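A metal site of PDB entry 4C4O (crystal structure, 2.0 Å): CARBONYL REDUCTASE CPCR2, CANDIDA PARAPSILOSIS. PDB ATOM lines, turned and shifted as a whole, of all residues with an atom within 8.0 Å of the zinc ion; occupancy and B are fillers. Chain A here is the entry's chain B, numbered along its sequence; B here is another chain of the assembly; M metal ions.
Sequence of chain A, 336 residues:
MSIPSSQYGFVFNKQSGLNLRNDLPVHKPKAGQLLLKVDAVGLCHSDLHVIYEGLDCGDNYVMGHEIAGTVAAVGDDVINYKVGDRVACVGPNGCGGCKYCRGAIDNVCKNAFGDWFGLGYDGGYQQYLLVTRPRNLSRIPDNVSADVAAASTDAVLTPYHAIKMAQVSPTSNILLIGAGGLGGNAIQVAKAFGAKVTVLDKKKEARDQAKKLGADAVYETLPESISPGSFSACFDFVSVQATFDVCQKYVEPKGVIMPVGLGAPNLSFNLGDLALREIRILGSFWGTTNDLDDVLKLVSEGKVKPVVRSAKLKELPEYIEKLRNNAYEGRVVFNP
The side-chain sulfur (SG) of Cys 109 sits close to the backbone NH (N) of Asn 111 (3.6 Å). The side-chain sulfur (SG) of Cys 109 lies close to the backbone NH (N) of Ala 112 (3.7 Å). The side-chain sulfur (SG) of Cys 101 sits close to the backbone NH (N) of Gly 96 (3.3 Å). ND2 of Asn 111 lies close to SG of Cys 95, 3.4 Å away. SG of Cys 98 lies close to N of Tyr 100. The side-chain amide nitrogen of Asn 80 of chain B lies close to the side-chain sulfur of Cys 95 (3.6 Å). SG of Cys 95 lies close to N of Gly 97 (3.3 Å).
N of Gly 96 touches the zinc ion (3.8 Å). Of the 22 residues printed, 5 come within 4 Å of the zinc ion. The nearest printed residue that does not touch the zinc ion is Asn 111 (4.4 Å).
The zinc ion is bound by the side-chain sulfur of Cys 109 (2.3 Å), the side-chain sulfur of Cys 98 (2.3 Å), the side-chain sulfur of Cys 101 (2.3 Å) and the side-chain sulfur of Cys 95 (2.4 Å). The zinc ion has four donor atoms within binding distance.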
ATOM      1  N   PRO A  92       3.207  31.125  29.442  1.00  0.00           N
ATOM      2  CA  PRO A  92       4.201  30.113  29.925  1.00  0.00           C
ATOM      3  C   PRO A  92       4.762  29.263  28.806  1.00  0.00           C
ATOM      4  O   PRO A  92       5.753  28.566  29.034  1.00  0.00           O
ATOM      5  CB  PRO A  92       3.378  29.254  30.899  1.00  0.00           C
ATOM      6  CG  PRO A  92       2.384  30.269  31.448  1.00  0.00           C
ATOM      7  CD  PRO A  92       1.965  31.055  30.227  1.00  0.00           C
ATOM      8  N   ASN A  93       4.112  29.279  27.656  1.00  0.00           N
ATOM      9  CA  ASN A  93       4.712  28.690  26.440  1.00  0.00           C
ATOM     10  C   ASN A  93       5.176  27.242  26.734  1.00  0.00           C
ATOM     11  O   ASN A  93       6.264  26.907  26.419  1.00  0.00           O
ATOM     12  CB  ASN A  93       5.870  29.595  26.045  1.00  0.00           C
ATOM     13  CG  ASN A  93       6.393  29.392  24.616  1.00  0.00           C
ATOM     14  OD1 ASN A  93       7.591  29.725  24.281  1.00  0.00           O
ATOM     15  ND2 ASN A  93       5.609  28.815  23.799  1.00  0.00           N
ATOM     16  N   GLY A  94       4.341  26.392  27.335  1.00  0.00           N
ATOM     17  CA  GLY A  94       4.719  24.995  27.718  1.00  0.00           C
ATOM     18  C   GLY A  94       5.185  24.137  26.534  1.00  0.00           C
ATOM     19  O   GLY A  94       4.791  24.363  25.378  1.00  0.00           O
ATOM     20  N   CYS A  95       6.029  23.141  26.817  1.00  0.00           N
ATOM     21  CA  CYS A  95       6.539  22.226  25.762  1.00  0.00           C
ATOM     22  C   CYS A  95       5.484  21.350  25.129  1.00  0.00           C
ATOM     23  O   CYS A  95       5.615  20.976  23.963  1.00  0.00           O
ATOM     24  CB  CYS A  95       7.690  21.389  26.358  1.00  0.00           C
ATOM     25  SG  CYS A  95       7.160  20.002  27.357  1.00  0.00           S
ATOM     26  N   GLY A  96       4.411  21.024  25.830  1.00  0.00           N
ATOM     27  CA  GLY A  96       3.361  20.157  25.263  1.00  0.00           C
ATOM     28  C   GLY A  96       3.552  18.646  25.469  1.00  0.00           C
ATOM     29  O   GLY A  96       2.624  17.862  25.322  1.00  0.00           O
ATOM     30  N   GLY A  97       4.769  18.233  25.848  1.00  0.00           N
ATOM     31  CA  GLY A  97       5.122  16.818  25.844  1.00  0.00           C
ATOM     32  C   GLY A  97       5.468  16.188  27.185  1.00  0.00           C
ATOM     33  O   GLY A  97       5.680  14.982  27.260  1.00  0.00           O
ATOM     34  N   CYS A  98       5.637  17.000  28.220  1.00  0.00           N
ATOM     35  CA  CYS A  98       6.044  16.507  29.525  1.00  0.00           C
ATOM     36  C   CYS A  98       4.825  16.146  30.357  1.00  0.00           C
ATOM     37  O   CYS A  98       3.672  16.380  29.946  1.00  0.00           O
ATOM     38  CB  CYS A  98       6.908  17.549  30.223  1.00  0.00           C
ATOM     39  SG  CYS A  98       5.969  18.970  30.814  1.00  0.00           S
ATOM     40  N   LYS A  99       5.068  15.595  31.544  1.00  0.00           N
ATOM     41  CA  LYS A  99       3.978  15.172  32.430  1.00  0.00           C
ATOM     42  C   LYS A  99       3.152  16.350  32.931  1.00  0.00           C
ATOM     43  O   LYS A  99       1.944  16.214  33.124  1.00  0.00           O
ATOM     44  CB  LYS A  99       4.475  14.363  33.627  1.00  0.00           C
ATOM     45  CG  LYS A  99       5.346  15.109  34.626  1.00  0.00           C
ATOM     46  CD  LYS A  99       5.772  14.164  35.759  1.00  0.00           C
ATOM     47  CE  LYS A  99       6.559  14.872  36.850  1.00  0.00           C
ATOM     48  NZ  LYS A  99       6.672  14.035  38.081  1.00  0.00           N
ATOM     49  N   TYR A 100       3.789  17.509  33.122  1.00  0.00           N
ATOM     50  CA  TYR A 100       3.022  18.676  33.562  1.00  0.00           C
ATOM     51  C   TYR A 100       2.100  19.141  32.460  1.00  0.00           C
ATOM     52  O   TYR A 100       0.900  19.315  32.689  1.00  0.00           O
ATOM     53  CB  TYR A 100       3.922  19.765  34.049  1.00  0.00           C
ATOM     54  CG  TYR A 100       4.778  19.332  35.188  1.00  0.00           C
ATOM     55  CD1 TYR A 100       4.265  19.116  36.459  1.00  0.00           C
ATOM     56  CD2 TYR A 100       6.124  19.072  34.968  1.00  0.00           C
ATOM     57  CE1 TYR A 100       5.081  18.696  37.499  1.00  0.00           C
ATOM     58  CE2 TYR A 100       6.957  18.657  36.004  1.00  0.00           C
ATOM     59  CZ  TYR A 100       6.431  18.492  37.248  1.00  0.00           C
ATOM     60  OH  TYR A 100       7.271  18.032  38.218  1.00  0.00           O
ATOM     61  N   CYS A 101       2.617  19.218  31.230  1.00  0.00           N
ATOM     62  CA  CYS A 101       1.814  19.657  30.085  1.00  0.00           C
ATOM     63  C   CYS A 101       0.689  18.675  29.724  1.00  0.00           C
ATOM     64  O   CYS A 101      -0.407  19.095  29.305  1.00  0.00           O
ATOM     65  CB  CYS A 101       2.686  19.950  28.859  1.00  0.00           C
ATOM     66  SG  CYS A 101       3.789  21.395  29.040  1.00  0.00           S
ATOM     67  N   ARG A 102       0.863  17.382  30.012  1.00  0.00           N
ATOM     68  CA  ARG A 102      -0.109  16.357  29.589  1.00  0.00           C
ATOM     69  C   ARG A 102      -1.394  15.927  30.379  1.00  0.00           C
ATOM     70  O   ARG A 102      -2.321  15.410  29.726  1.00  0.00           O
ATOM     71  CB  ARG A 102       0.661  15.056  29.250  1.00  0.00           C
ATOM     72  CG  ARG A 102       1.454  15.160  27.978  1.00  0.00           C
ATOM     73  CD  ARG A 102       2.019  13.811  27.600  1.00  0.00           C
ATOM     74  NE  ARG A 102       2.366  13.031  28.789  1.00  0.00           N
ATOM     75  CZ  ARG A 102       3.517  12.428  29.015  1.00  0.00           C
ATOM     76  NH1 ARG A 102       4.489  12.438  28.104  1.00  0.00           N
ATOM     77  NH2 ARG A 102       3.697  11.815  30.153  1.00  0.00           N
ATOM     78  N   ILE A 105      -1.421  21.051  33.428  1.00  0.00           N
ATOM     79  CA  ILE A 105      -0.700  22.058  34.161  1.00  0.00           C
ATOM     80  C   ILE A 105       0.500  22.494  33.336  1.00  0.00           C
ATOM     81  O   ILE A 105       1.630  22.515  33.806  1.00  0.00           O
ATOM     82  CB  ILE A 105      -0.347  21.604  35.595  1.00  0.00           C
ATOM     83  CG1 ILE A 105       0.373  20.258  35.604  1.00  0.00           C
ATOM     84  CG2 ILE A 105      -1.618  21.445  36.444  1.00  0.00           C
ATOM     85  CD1 ILE A 105       0.684  19.710  37.009  1.00  0.00           C
ATOM     86  N   ASP A 106       0.191  23.013  32.140  1.00  0.00           N
ATOM     87  CA  ASP A 106       1.259  23.468  31.235  1.00  0.00           C
ATOM     88  C   ASP A 106       1.903  24.746  31.704  1.00  0.00           C
ATOM     89  O   ASP A 106       2.936  25.132  31.199  1.00  0.00           O
ATOM     90  CB  ASP A 106       0.865  23.487  29.751  1.00  0.00           C
ATOM     91  CG  ASP A 106      -0.413  24.298  29.466  1.00  0.00           C
ATOM     92  OD1 ASP A 106      -0.803  25.162  30.276  1.00  0.00           O
ATOM     93  OD2 ASP A 106      -0.956  24.128  28.346  1.00  0.00           O
ATOM     94  N   ASN A 107       1.327  25.375  32.727  1.00  0.00           N
ATOM     95  CA  ASN A 107       1.978  26.552  33.315  1.00  0.00           C
ATOM     96  C   ASN A 107       3.228  26.268  34.129  1.00  0.00           C
ATOM     97  O   ASN A 107       3.991  27.204  34.406  1.00  0.00           O
ATOM     98  CB  ASN A 107       0.982  27.378  34.137  1.00  0.00           C
ATOM     99  CG  ASN A 107       0.361  26.604  35.280  1.00  0.00           C
ATOM    100  OD1 ASN A 107       0.025  25.443  35.140  1.00  0.00           O
ATOM    101  ND2 ASN A 107       0.203  27.256  36.414  1.00  0.00           N
ATOM    102  N   VAL A 108       3.418  25.035  34.590  1.00  0.00           N
ATOM    103  CA  VAL A 108       4.575  24.723  35.418  1.00  0.00           C
ATOM    104  C   VAL A 108       5.486  23.737  34.689  1.00  0.00           C
ATOM    105  O   VAL A 108       6.248  23.040  35.318  1.00  0.00           O
ATOM    106  CB  VAL A 108       4.216  24.139  36.831  1.00  0.00           C
ATOM    107  CG1 VAL A 108       3.432  25.127  37.659  1.00  0.00           C
ATOM    108  CG2 VAL A 108       3.466  22.807  36.753  1.00  0.00           C
ATOM    109  N   CYS A 109       5.438  23.758  33.369  1.00  0.00           N
ATOM    110  CA  CYS A 109       6.380  23.049  32.554  1.00  0.00           C
ATOM    111  C   CYS A 109       7.839  23.338  32.887  1.00  0.00           C
ATOM    112  O   CYS A 109       8.336  24.446  32.652  1.00  0.00           O
ATOM    113  CB  CYS A 109       6.134  23.391  31.106  1.00  0.00           C
ATOM    114  SG  CYS A 109       7.155  22.536  29.876  1.00  0.00           S
ATOM    115  N   LYS A 110       8.585  22.316  33.312  1.00  0.00           N
ATOM    116  CA  LYS A 110      10.053  22.456  33.580  1.00  0.00           C
ATOM    117  C   LYS A 110      10.827  22.766  32.339  1.00  0.00           C
ATOM    118  O   LYS A 110      11.728  23.630  32.355  1.00  0.00           O
ATOM    119  CB  LYS A 110      10.650  21.201  34.246  1.00  0.00           C
ATOM    120  N   ASN A 111      10.492  22.154  31.226  1.00  0.00           N
ATOM    121  CA  ASN A 111      11.195  22.444  29.971  1.00  0.00           C
ATOM    122  C   ASN A 111      11.141  23.891  29.485  1.00  0.00           C
ATOM    123  O   ASN A 111      11.927  24.272  28.632  1.00  0.00           O
ATOM    124  CB  ASN A 111      10.748  21.492  28.847  1.00  0.00           C
ATOM    125  CG  ASN A 111      10.983  20.021  29.200  1.00  0.00           C
ATOM    126  OD1 ASN A 111      11.927  19.704  29.916  1.00  0.00           O
ATOM    127  ND2 ASN A 111      10.084  19.145  28.783  1.00  0.00           N
ATOM    128  N   ALA A 112      10.154  24.642  29.948  1.00  0.00           N
ATOM    129  CA  ALA A 112       9.906  25.952  29.387  1.00  0.00           C
ATOM    130  C   ALA A 112      10.413  27.046  30.313  1.00  0.00           C
ATOM    131  O   ALA A 112      10.287  28.201  30.010  1.00  0.00           O
ATOM    132  CB  ALA A 112       8.406  26.119  29.084  1.00  0.00           C
ATOM    133  N   ARG A 133       5.819  27.384  19.140  1.00  0.00           N
ATOM    134  CA  ARG A 133       4.862  26.355  19.553  1.00  0.00           C
ATOM    135  C   ARG A 133       3.442  26.890  19.473  1.00  0.00           C
ATOM    136  O   ARG A 133       2.946  27.483  20.433  1.00  0.00           O
ATOM    137  CB  ARG A 133       5.173  25.886  20.975  1.00  0.00           C
ATOM    138  CG  ARG A 133       6.464  25.099  21.104  1.00  0.00           C
ATOM    139  CD  ARG A 133       6.839  24.891  22.563  1.00  0.00           C
ATOM    140  NE  ARG A 133       7.975  25.728  22.963  1.00  0.00           N
ATOM    141  CZ  ARG A 133       8.278  26.035  24.217  1.00  0.00           C
ATOM    142  NH1 ARG A 133       7.538  25.561  25.208  1.00  0.00           N
ATOM    143  NH2 ARG A 133       9.328  26.802  24.484  1.00  0.00           N
ATOM    144  N   ARG A 135       0.680  25.438  19.726  1.00  0.00           N
ATOM    145  CA  ARG A 135      -0.222  24.942  20.744  1.00  0.00           C
ATOM    146  C   ARG A 135      -0.506  26.018  21.809  1.00  0.00           C
ATOM    147  O   ARG A 135      -1.531  25.983  22.444  1.00  0.00           O
ATOM    148  CB  ARG A 135       0.327  23.672  21.450  1.00  0.00           C
ATOM    149  CG  ARG A 135       1.431  23.924  22.487  1.00  0.00           C
ATOM    150  CD  ARG A 135       1.733  22.693  23.360  1.00  0.00           C
ATOM    151  NE  ARG A 135       1.103  22.765  24.691  1.00  0.00           N
ATOM    152  CZ  ARG A 135       0.271  21.897  25.194  1.00  0.00           C
ATOM    153  NH1 ARG A 135      -0.147  20.858  24.471  1.00  0.00           N
ATOM    154  NH2 ARG A 135      -0.189  22.085  26.434  1.00  0.00           N
ATOM    155  N   ASN B  80      11.679  16.356  24.496  1.00  0.00           N
ATOM    156  CA  ASN B  80      11.391  15.456  25.599  1.00  0.00           C
ATOM    157  C   ASN B  80      12.009  14.051  25.451  1.00  0.00           C
ATOM    158  O   ASN B  80      12.100  13.324  26.429  1.00  0.00           O
ATOM    159  CB  ASN B  80       9.893  15.317  25.782  1.00  0.00           C
ATOM    160  CG  ASN B  80       9.246  16.595  26.292  1.00  0.00           C
ATOM    161  OD1 ASN B  80       9.275  16.901  27.502  1.00  0.00           O
ATOM    162  ND2 ASN B  80       8.640  17.344  25.382  1.00  0.00           N
HETATM  163 ZN    ZN M   1       5.999  20.693  29.284  1.00  0.00          ZN
